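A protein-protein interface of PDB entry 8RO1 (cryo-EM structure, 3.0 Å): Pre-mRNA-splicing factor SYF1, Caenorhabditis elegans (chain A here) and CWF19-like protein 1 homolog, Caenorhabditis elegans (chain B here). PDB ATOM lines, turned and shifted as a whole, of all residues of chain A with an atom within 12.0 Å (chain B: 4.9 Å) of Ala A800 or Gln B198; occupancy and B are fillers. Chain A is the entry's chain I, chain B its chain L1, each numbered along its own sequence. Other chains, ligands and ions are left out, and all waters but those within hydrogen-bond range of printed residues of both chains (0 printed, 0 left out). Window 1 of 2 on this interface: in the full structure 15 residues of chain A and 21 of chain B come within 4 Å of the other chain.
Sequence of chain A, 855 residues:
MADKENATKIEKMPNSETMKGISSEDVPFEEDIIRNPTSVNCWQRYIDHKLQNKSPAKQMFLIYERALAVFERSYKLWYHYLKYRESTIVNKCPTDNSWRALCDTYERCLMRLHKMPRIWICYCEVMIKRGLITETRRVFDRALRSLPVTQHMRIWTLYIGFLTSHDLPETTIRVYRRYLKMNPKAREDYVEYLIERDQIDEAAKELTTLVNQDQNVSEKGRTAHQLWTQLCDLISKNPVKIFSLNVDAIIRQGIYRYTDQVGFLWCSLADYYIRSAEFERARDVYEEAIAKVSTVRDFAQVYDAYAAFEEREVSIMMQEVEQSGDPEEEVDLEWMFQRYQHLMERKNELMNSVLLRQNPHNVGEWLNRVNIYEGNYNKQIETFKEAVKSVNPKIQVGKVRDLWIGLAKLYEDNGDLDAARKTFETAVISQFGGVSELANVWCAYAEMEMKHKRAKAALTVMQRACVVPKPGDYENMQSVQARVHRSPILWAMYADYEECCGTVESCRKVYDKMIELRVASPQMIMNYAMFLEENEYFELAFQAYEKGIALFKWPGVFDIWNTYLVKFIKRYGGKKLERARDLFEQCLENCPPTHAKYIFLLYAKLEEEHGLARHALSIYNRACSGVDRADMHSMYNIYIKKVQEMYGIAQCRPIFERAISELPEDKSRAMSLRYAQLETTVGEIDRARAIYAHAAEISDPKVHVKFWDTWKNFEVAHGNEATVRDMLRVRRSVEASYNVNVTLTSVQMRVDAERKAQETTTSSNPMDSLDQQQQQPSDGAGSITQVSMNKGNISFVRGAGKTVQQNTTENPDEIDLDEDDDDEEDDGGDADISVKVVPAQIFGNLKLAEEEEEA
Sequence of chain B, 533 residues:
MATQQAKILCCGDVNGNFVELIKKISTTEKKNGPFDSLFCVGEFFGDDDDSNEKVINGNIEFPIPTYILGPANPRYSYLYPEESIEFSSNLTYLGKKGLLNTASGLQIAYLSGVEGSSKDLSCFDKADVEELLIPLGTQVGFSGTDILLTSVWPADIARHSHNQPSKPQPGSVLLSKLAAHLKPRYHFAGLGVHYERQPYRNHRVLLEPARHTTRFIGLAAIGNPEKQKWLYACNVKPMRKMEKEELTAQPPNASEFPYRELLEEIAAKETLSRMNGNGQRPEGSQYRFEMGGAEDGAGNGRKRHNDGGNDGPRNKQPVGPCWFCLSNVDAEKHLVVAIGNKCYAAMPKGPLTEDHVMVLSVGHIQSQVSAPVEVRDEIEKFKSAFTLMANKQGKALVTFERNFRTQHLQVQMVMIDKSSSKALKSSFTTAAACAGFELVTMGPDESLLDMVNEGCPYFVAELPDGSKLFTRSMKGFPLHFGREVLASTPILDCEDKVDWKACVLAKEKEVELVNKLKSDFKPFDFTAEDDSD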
ATOM      1  N   ASN A 790      27.303   6.515  35.760  1.00  0.00           N
ATOM      2  CA  ASN A 790      27.959   6.115  34.525  1.00  0.00           C
ATOM      3  C   ASN A 790      29.420   6.533  34.499  1.00  0.00           C
ATOM      4  O   ASN A 790      29.833   7.470  35.181  1.00  0.00           O
ATOM      5  CB  ASN A 790      27.255   6.715  33.315  1.00  0.00           C
ATOM      6  CG  ASN A 790      27.640   6.029  32.035  1.00  0.00           C
ATOM      7  OD1 ASN A 790      28.679   6.322  31.453  1.00  0.00           O
ATOM      8  ND2 ASN A 790      26.795   5.114  31.577  1.00  0.00           N
ATOM      9  N   GLY A 792      31.373   5.801  30.741  1.00  0.00           N
ATOM     10  CA  GLY A 792      31.617   5.046  29.521  1.00  0.00           C
ATOM     11  C   GLY A 792      32.829   5.511  28.731  1.00  0.00           C
ATOM     12  O   GLY A 792      33.226   6.672  28.800  1.00  0.00           O
ATOM     13  N   ASN A 793      33.420   4.577  27.981  1.00  0.00           N
ATOM     14  CA  ASN A 793      34.545   4.863  27.095  1.00  0.00           C
ATOM     15  C   ASN A 793      34.088   5.294  25.703  1.00  0.00           C
ATOM     16  O   ASN A 793      33.097   4.786  25.173  1.00  0.00           O
ATOM     17  CB  ASN A 793      35.438   3.629  26.955  1.00  0.00           C
ATOM     18  CG  ASN A 793      36.062   3.203  28.267  1.00  0.00           C
ATOM     19  OD1 ASN A 793      36.217   4.006  29.186  1.00  0.00           O
ATOM     20  ND2 ASN A 793      36.428   1.930  28.357  1.00  0.00           N
ATOM     21  N   ILE A 794      34.829   6.241  25.117  1.00  0.00           N
ATOM     22  CA  ILE A 794      34.536   6.733  23.772  1.00  0.00           C
ATOM     23  C   ILE A 794      34.840   5.638  22.759  1.00  0.00           C
ATOM     24  O   ILE A 794      35.844   4.923  22.877  1.00  0.00           O
ATOM     25  CB  ILE A 794      35.337   8.019  23.481  1.00  0.00           C
ATOM     26  CG1 ILE A 794      34.790   9.185  24.313  1.00  0.00           C
ATOM     27  CG2 ILE A 794      35.325   8.404  21.963  1.00  0.00           C
ATOM     28  CD1 ILE A 794      35.730  10.380  24.419  1.00  0.00           C
ATOM     29  N   SER A 795      33.975   5.509  21.749  1.00  0.00           N
ATOM     30  CA  SER A 795      34.289   4.679  20.590  1.00  0.00           C
ATOM     31  C   SER A 795      35.105   5.486  19.577  1.00  0.00           C
ATOM     32  O   SER A 795      36.336   5.381  19.571  1.00  0.00           O
ATOM     33  CB  SER A 795      33.004   4.094  19.973  1.00  0.00           C
ATOM     34  OG  SER A 795      32.102   3.655  20.974  1.00  0.00           O
ATOM     35  N   PHE A 796      34.459   6.292  18.732  1.00  0.00           N
ATOM     36  CA  PHE A 796      35.155   7.090  17.734  1.00  0.00           C
ATOM     37  C   PHE A 796      34.558   8.482  17.698  1.00  0.00           C
ATOM     38  O   PHE A 796      33.382   8.684  18.003  1.00  0.00           O
ATOM     39  CB  PHE A 796      35.049   6.488  16.329  1.00  0.00           C
ATOM     40  CG  PHE A 796      35.563   5.080  16.223  1.00  0.00           C
ATOM     41  CD1 PHE A 796      36.922   4.825  16.186  1.00  0.00           C
ATOM     42  CD2 PHE A 796      34.682   4.015  16.158  1.00  0.00           C
ATOM     43  CE1 PHE A 796      37.395   3.529  16.085  1.00  0.00           C
ATOM     44  CE2 PHE A 796      35.147   2.719  16.057  1.00  0.00           C
ATOM     45  CZ  PHE A 796      36.506   2.474  16.021  1.00  0.00           C
ATOM     46  N   VAL A 797      35.393   9.440  17.329  1.00  0.00           N
ATOM     47  CA  VAL A 797      34.942  10.697  16.754  1.00  0.00           C
ATOM     48  C   VAL A 797      34.362  10.433  15.362  1.00  0.00           C
ATOM     49  O   VAL A 797      35.117  10.301  14.393  1.00  0.00           O
ATOM     50  CB  VAL A 797      36.114  11.703  16.719  1.00  0.00           C
ATOM     51  CG1 VAL A 797      35.732  12.964  16.019  1.00  0.00           C
ATOM     52  CG2 VAL A 797      36.575  12.053  18.133  1.00  0.00           C
ATOM     53  N   ARG A 798      33.028  10.356  15.249  1.00  0.00           N
ATOM     54  CA  ARG A 798      32.370   9.807  14.061  1.00  0.00           C
ATOM     55  C   ARG A 798      31.113  10.604  13.709  1.00  0.00           C
ATOM     56  O   ARG A 798      31.081  11.811  13.969  1.00  0.00           O
ATOM     57  CB  ARG A 798      32.114   8.309  14.281  1.00  0.00           C
ATOM     58  CG  ARG A 798      32.737   7.395  13.222  1.00  0.00           C
ATOM     59  CD  ARG A 798      32.221   7.677  11.809  1.00  0.00           C
ATOM     60  NE  ARG A 798      32.774   6.748  10.827  1.00  0.00           N
ATOM     61  CZ  ARG A 798      33.944   6.880  10.210  1.00  0.00           C
ATOM     62  NH1 ARG A 798      34.311   5.962   9.321  1.00  0.00           N
ATOM     63  NH2 ARG A 798      34.757   7.898  10.456  1.00  0.00           N
ATOM     64  N   GLY A 799      30.088   9.991  13.105  1.00  0.00           N
ATOM     65  CA  GLY A 799      28.950  10.777  12.674  1.00  0.00           C
ATOM     66  C   GLY A 799      27.680  10.086  12.215  1.00  0.00           C
ATOM     67  O   GLY A 799      26.930  10.704  11.453  1.00  0.00           O
ATOM     68  N   ALA A 800      27.403   8.846  12.624  1.00  0.00           N
ATOM     69  CA  ALA A 800      26.140   8.219  12.240  1.00  0.00           C
ATOM     70  C   ALA A 800      25.661   7.257  13.317  1.00  0.00           C
ATOM     71  O   ALA A 800      26.414   6.857  14.207  1.00  0.00           O
ATOM     72  CB  ALA A 800      26.263   7.480  10.901  1.00  0.00           C
ATOM     73  N   GLY A 801      24.379   6.902  13.222  1.00  0.00           N
ATOM     74  CA  GLY A 801      23.796   5.867  14.047  1.00  0.00           C
ATOM     75  C   GLY A 801      22.382   5.474  13.664  1.00  0.00           C
ATOM     76  O   GLY A 801      22.072   5.224  12.498  1.00  0.00           O
ATOM     77  N   LYS A 802      21.514   5.459  14.684  1.00  0.00           N
ATOM     78  CA  LYS A 802      20.266   4.690  14.726  1.00  0.00           C
ATOM     79  C   LYS A 802      19.304   4.917  13.566  1.00  0.00           C
ATOM     80  O   LYS A 802      18.412   4.084  13.371  1.00  0.00           O
ATOM     81  CB  LYS A 802      19.493   4.991  16.019  1.00  0.00           C
ATOM     82  CG  LYS A 802      18.742   3.810  16.646  1.00  0.00           C
ATOM     83  CD  LYS A 802      19.645   2.647  17.041  1.00  0.00           C
ATOM     84  CE  LYS A 802      19.480   1.461  16.099  1.00  0.00           C
ATOM     85  NZ  LYS A 802      20.592   0.484  16.223  1.00  0.00           N
ATOM     86  N   THR A 803      19.431   6.036  12.840  1.00  0.00           N
ATOM     87  CA  THR A 803      18.329   6.617  12.072  1.00  0.00           C
ATOM     88  C   THR A 803      17.645   5.640  11.125  1.00  0.00           C
ATOM     89  O   THR A 803      16.434   5.747  10.904  1.00  0.00           O
ATOM     90  CB  THR A 803      18.851   7.823  11.279  1.00  0.00           C
ATOM     91  OG1 THR A 803      18.920   8.950  12.154  1.00  0.00           O
ATOM     92  CG2 THR A 803      17.941   8.191  10.068  1.00  0.00           C
ATOM     93  N   VAL A 804      18.392   4.698  10.550  1.00  0.00           N
ATOM     94  CA  VAL A 804      17.783   3.707   9.665  1.00  0.00           C
ATOM     95  C   VAL A 804      16.767   2.860  10.427  1.00  0.00           C
ATOM     96  O   VAL A 804      15.666   2.592   9.928  1.00  0.00           O
ATOM     97  CB  VAL A 804      18.871   2.834   9.006  1.00  0.00           C
ATOM     98  CG1 VAL A 804      18.246   1.739   8.116  1.00  0.00           C
ATOM     99  CG2 VAL A 804      19.849   3.696   8.192  1.00  0.00           C
ATOM    100  N   GLN A 805      17.113   2.428  11.645  1.00  0.00           N
ATOM    101  CA  GLN A 805      16.121   1.809  12.522  1.00  0.00           C
ATOM    102  C   GLN A 805      15.157   2.817  13.141  1.00  0.00           C
ATOM    103  O   GLN A 805      14.010   2.461  13.431  1.00  0.00           O
ATOM    104  CB  GLN A 805      16.814   0.994  13.612  1.00  0.00           C
ATOM    105  CG  GLN A 805      17.633  -0.162  13.059  1.00  0.00           C
ATOM    106  CD  GLN A 805      17.974  -1.202  14.110  1.00  0.00           C
ATOM    107  OE1 GLN A 805      19.074  -1.210  14.661  1.00  0.00           O
ATOM    108  NE2 GLN A 805      17.027  -2.094  14.385  1.00  0.00           N
ATOM    109  N   GLN A 806      15.586   4.059  13.381  1.00  0.00           N
ATOM    110  CA  GLN A 806      14.652   5.031  13.939  1.00  0.00           C
ATOM    111  C   GLN A 806      13.580   5.407  12.931  1.00  0.00           C
ATOM    112  O   GLN A 806      12.420   5.608  13.301  1.00  0.00           O
ATOM    113  CB  GLN A 806      15.374   6.291  14.407  1.00  0.00           C
ATOM    114  CG  GLN A 806      14.502   7.311  15.160  1.00  0.00           C
ATOM    115  CD  GLN A 806      13.686   6.722  16.298  1.00  0.00           C
ATOM    116  OE1 GLN A 806      14.161   5.861  17.039  1.00  0.00           O
ATOM    117  NE2 GLN A 806      12.437   7.159  16.415  1.00  0.00           N
ATOM    118  N   ASN A 807      13.951   5.522  11.662  1.00  0.00           N
ATOM    119  CA  ASN A 807      12.984   5.717  10.591  1.00  0.00           C
ATOM    120  C   ASN A 807      12.012   4.546  10.533  1.00  0.00           C
ATOM    121  O   ASN A 807      12.258   3.560   9.836  1.00  0.00           O
ATOM    122  CB  ASN A 807      13.690   5.852   9.240  1.00  0.00           C
ATOM    123  CG  ASN A 807      14.397   7.179   9.077  1.00  0.00           C
ATOM    124  OD1 ASN A 807      14.352   8.032   9.961  1.00  0.00           O
ATOM    125  ND2 ASN A 807      15.036   7.372   7.927  1.00  0.00           N
ATOM    126  N   SER B 161      28.358   9.667  25.373  1.00  0.00           N
ATOM    127  CA  SER B 161      27.861   9.366  24.038  1.00  0.00           C
ATOM    128  C   SER B 161      28.715   8.238  23.466  1.00  0.00           C
ATOM    129  O   SER B 161      29.934   8.225  23.642  1.00  0.00           O
ATOM    130  CB  SER B 161      27.913  10.607  23.149  1.00  0.00           C
ATOM    131  OG  SER B 161      27.364  10.349  21.868  1.00  0.00           O
ATOM    132  N   HIS B 162      28.075   7.290  22.775  1.00  0.00           N
ATOM    133  CA  HIS B 162      28.822   6.138  22.277  1.00  0.00           C
ATOM    134  C   HIS B 162      29.718   6.502  21.107  1.00  0.00           C
ATOM    135  O   HIS B 162      30.629   5.739  20.779  1.00  0.00           O
ATOM    136  CB  HIS B 162      27.865   5.028  21.848  1.00  0.00           C
ATOM    137  CG  HIS B 162      26.968   4.545  22.943  1.00  0.00           C
ATOM    138  ND1 HIS B 162      27.444   4.035  24.131  1.00  0.00           N
ATOM    139  CD2 HIS B 162      25.617   4.490  23.024  1.00  0.00           C
ATOM    140  CE1 HIS B 162      26.426   3.694  24.900  1.00  0.00           C
ATOM    141  NE2 HIS B 162      25.306   3.958  24.252  1.00  0.00           N
ATOM    142  N   ASN B 163      29.469   7.643  20.479  1.00  0.00           N
ATOM    143  CA  ASN B 163      30.363   8.278  19.535  1.00  0.00           C
ATOM    144  C   ASN B 163      30.563   9.692  20.042  1.00  0.00           C
ATOM    145  O   ASN B 163      29.873  10.126  20.962  1.00  0.00           O
ATOM    146  CB  ASN B 163      29.813   8.226  18.105  1.00  0.00           C
ATOM    147  CG  ASN B 163      28.452   8.888  17.962  1.00  0.00           C
ATOM    148  OD1 ASN B 163      27.917   9.473  18.905  1.00  0.00           O
ATOM    149  ND2 ASN B 163      27.876   8.787  16.770  1.00  0.00           N
ATOM    150  N   GLU B 196      24.611  13.064  14.187  1.00  0.00           N
ATOM    151  CA  GLU B 196      23.748  12.098  14.851  1.00  0.00           C
ATOM    152  C   GLU B 196      24.450  11.659  16.131  1.00  0.00           C
ATOM    153  O   GLU B 196      25.285  10.754  16.108  1.00  0.00           O
ATOM    154  CB  GLU B 196      23.463  10.927  13.920  1.00  0.00           C
ATOM    155  CG  GLU B 196      22.483   9.914  14.478  1.00  0.00           C
ATOM    156  CD  GLU B 196      21.997   8.944  13.425  1.00  0.00           C
ATOM    157  OE1 GLU B 196      22.702   8.775  12.407  1.00  0.00           O
ATOM    158  OE2 GLU B 196      20.919   8.342  13.614  1.00  0.00           O
ATOM    159  N   ARG B 197      24.133  12.290  17.259  1.00  0.00           N
ATOM    160  CA  ARG B 197      24.335  11.622  18.538  1.00  0.00           C
ATOM    161  C   ARG B 197      23.431  10.404  18.654  1.00  0.00           C
ATOM    162  O   ARG B 197      22.260  10.443  18.274  1.00  0.00           O
ATOM    163  CB  ARG B 197      24.041  12.560  19.699  1.00  0.00           C
ATOM    164  CG  ARG B 197      24.576  12.053  21.020  1.00  0.00           C
ATOM    165  CD  ARG B 197      23.601  12.286  22.139  1.00  0.00           C
ATOM    166  NE  ARG B 197      24.238  12.138  23.443  1.00  0.00           N
ATOM    167  CZ  ARG B 197      24.197  11.050  24.205  1.00  0.00           C
ATOM    168  NH1 ARG B 197      24.772  11.079  25.403  1.00  0.00           N
ATOM    169  NH2 ARG B 197      23.618   9.926  23.801  1.00  0.00           N
ATOM    170  N   GLN B 198      23.970   9.325  19.201  1.00  0.00           N
ATOM    171  CA  GLN B 198      23.175   8.152  19.472  1.00  0.00           C
ATOM    172  C   GLN B 198      22.255   8.482  20.644  1.00  0.00           C
ATOM    173  O   GLN B 198      22.458   9.486  21.317  1.00  0.00           O
ATOM    174  CB  GLN B 198      24.097   6.968  19.754  1.00  0.00           C
ATOM    175  CG  GLN B 198      25.054   6.686  18.604  1.00  0.00           C
ATOM    176  CD  GLN B 198      25.620   5.273  18.617  1.00  0.00           C
ATOM    177  OE1 GLN B 198      25.343   4.480  19.518  1.00  0.00           O
ATOM    178  NE2 GLN B 198      26.404   4.947  17.595  1.00  0.00           N
ATOM    179  N   PRO B 199      21.234   7.664  20.929  1.00  0.00           N
ATOM    180  CA  PRO B 199      20.210   8.089  21.902  1.00  0.00           C
ATOM    181  C   PRO B 199      20.700   8.366  23.320  1.00  0.00           C
ATOM    182  O   PRO B 199      21.883   8.209  23.621  1.00  0.00           O
ATOM    183  CB  PRO B 199      19.222   6.917  21.901  1.00  0.00           C
ATOM    184  CG  PRO B 199      19.449   6.207  20.649  1.00  0.00           C
ATOM    185  CD  PRO B 199      20.872   6.389  20.288  1.00  0.00           C
ATOM    186  N   TYR B 200      19.796   8.824  24.188  1.00  0.00           N
ATOM    187  CA  TYR B 200      20.025   8.792  25.626  1.00  0.00           C
ATOM    188  C   TYR B 200      18.699   8.689  26.366  1.00  0.00           C
ATOM    189  O   TYR B 200      17.671   9.192  25.913  1.00  0.00           O
ATOM    190  CB  TYR B 200      20.788  10.011  26.126  1.00  0.00           C
ATOM    191  CG  TYR B 200      20.176  11.326  25.749  1.00  0.00           C
ATOM    192  CD1 TYR B 200      19.223  11.924  26.549  1.00  0.00           C
ATOM    193  CD2 TYR B 200      20.585  11.996  24.612  1.00  0.00           C
ATOM    194  CE1 TYR B 200      18.677  13.136  26.219  1.00  0.00           C
ATOM    195  CE2 TYR B 200      20.043  13.216  24.272  1.00  0.00           C
ATOM    196  CZ  TYR B 200      19.084  13.778  25.077  1.00  0.00           C
ATOM    197  OH  TYR B 200      18.540  14.997  24.749  1.00  0.00           O
ATOM    198  N   ASN B 253      20.657   1.361  21.292  1.00  0.00           N
ATOM    199  CA  ASN B 253      21.900   2.084  21.524  1.00  0.00           C
ATOM    200  C   ASN B 253      21.804   3.098  22.660  1.00  0.00           C
ATOM    201  O   ASN B 253      22.538   4.095  22.665  1.00  0.00           O
ATOM    202  CB  ASN B 253      22.341   2.740  20.219  1.00  0.00           C
ATOM    203  CG  ASN B 253      22.797   1.722  19.210  1.00  0.00           C
ATOM    204  OD1 ASN B 253      21.988   0.989  18.651  1.00  0.00           O
ATOM    205  ND2 ASN B 253      24.101   1.652  18.984  1.00  0.00           N
ATOM    206  N   SER B 255      21.962   5.418  25.805  1.00  0.00           N
ATOM    207  CA  SER B 255      22.930   5.900  26.780  1.00  0.00           C
ATOM    208  C   SER B 255      22.244   6.571  27.970  1.00  0.00           C
ATOM    209  O   SER B 255      21.041   6.819  27.965  1.00  0.00           O
ATOM    210  CB  SER B 255      23.929   6.858  26.121  1.00  0.00           C
ATOM    211  OG  SER B 255      23.302   7.983  25.532  1.00  0.00           O
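OG of Ser A795 is in hydrogen-bond range of O of His B162 (2.6 Å).
N of Gly A801 lies within hydrogen-bond range of OE1 of Glu B196, 2.6 Å away.
OE2 of Glu B196 sits at hydrogen-bond distance from N of Lys A802, at 3.1 Å.
OE2 of Glu B196 lies within hydrogen-bond range of OG1 of Thr A803 (2.5 Å).
NZ of Lys A802 sits at hydrogen-bond distance from OD1 of Asn B253, at 2.8 Å.
OG of Ser B161 sits at hydrogen-bond distance from O of Asn B163 (2.7 Å).
The backbone carbonyl oxygen (O) of Asn B253 lies close to a ring nitrogen (NE2) of His B162 (3.2 Å).
O of Glu B196 lies within hydrogen-bond range of ND2 of Asn B163 (3.3 Å).
The side-chain amide oxygen (OE1) of Gln B198 is in hydrogen-bond range of the side-chain amide nitrogen (ND2) of Asn B253 (3.1 Å).
NZ of Lys A802 lies within hydrogen-bond range of OE1 of Gln A805 (2.8 Å).
O of Thr A803 sits close to OD1 of Asn A807 (3.2 Å).
Among the printed residues, pairs that only touch across the chains: Phe A796 with Asn B163 (3.4 Å), Ala A800 with Glu B196 (3.4 Å), Ala A800 with Asn B163 (3.5 Å) and Ala A800 with Gln B198 (3.9 Å).
Ala A800 touches three residues of chain B.
Of the printed residues of chain A, Gln B198 touches Ala A800.
Asn B163 touches two residues of chain A.
Glu B196 touches just these residues of chain A: Ala A800, Gly A801, Lys A802 and Thr A803.
No residue of chain A comes within 4 Å of Arg B197.
No residue of chain A comes within 4 Å of Pro B199.
No residue of chain A comes within 4 Å of Tyr B200.
Asn B253 touches just one residue of chain A: Lys A802 (2.8 Å).
No residue of chain A comes within 4 Å of Ser B255.
Printed residues of chain B within 4 Å of Ser A795: His B162 (2.6 Å).
Printed residues of chain B within 4 Å of Gly A801: Glu B196.
The nearest printed residue of chain B that does not touch Ala A800 is Arg B197 (6.4 Å).
The nearest printed residue of chain B that does not touch Lys A802 is Pro B199 (4.7 Å).
Of the 17 printed residues of chain A, 6 touch a printed residue of chain B.
Among the printed residues, 9 pairs touch across the chains.
Among the printed residues, no Asp or Glu carboxylate lies within 4 Å of a Lys or Arg side-chain nitrogen of the other chain.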
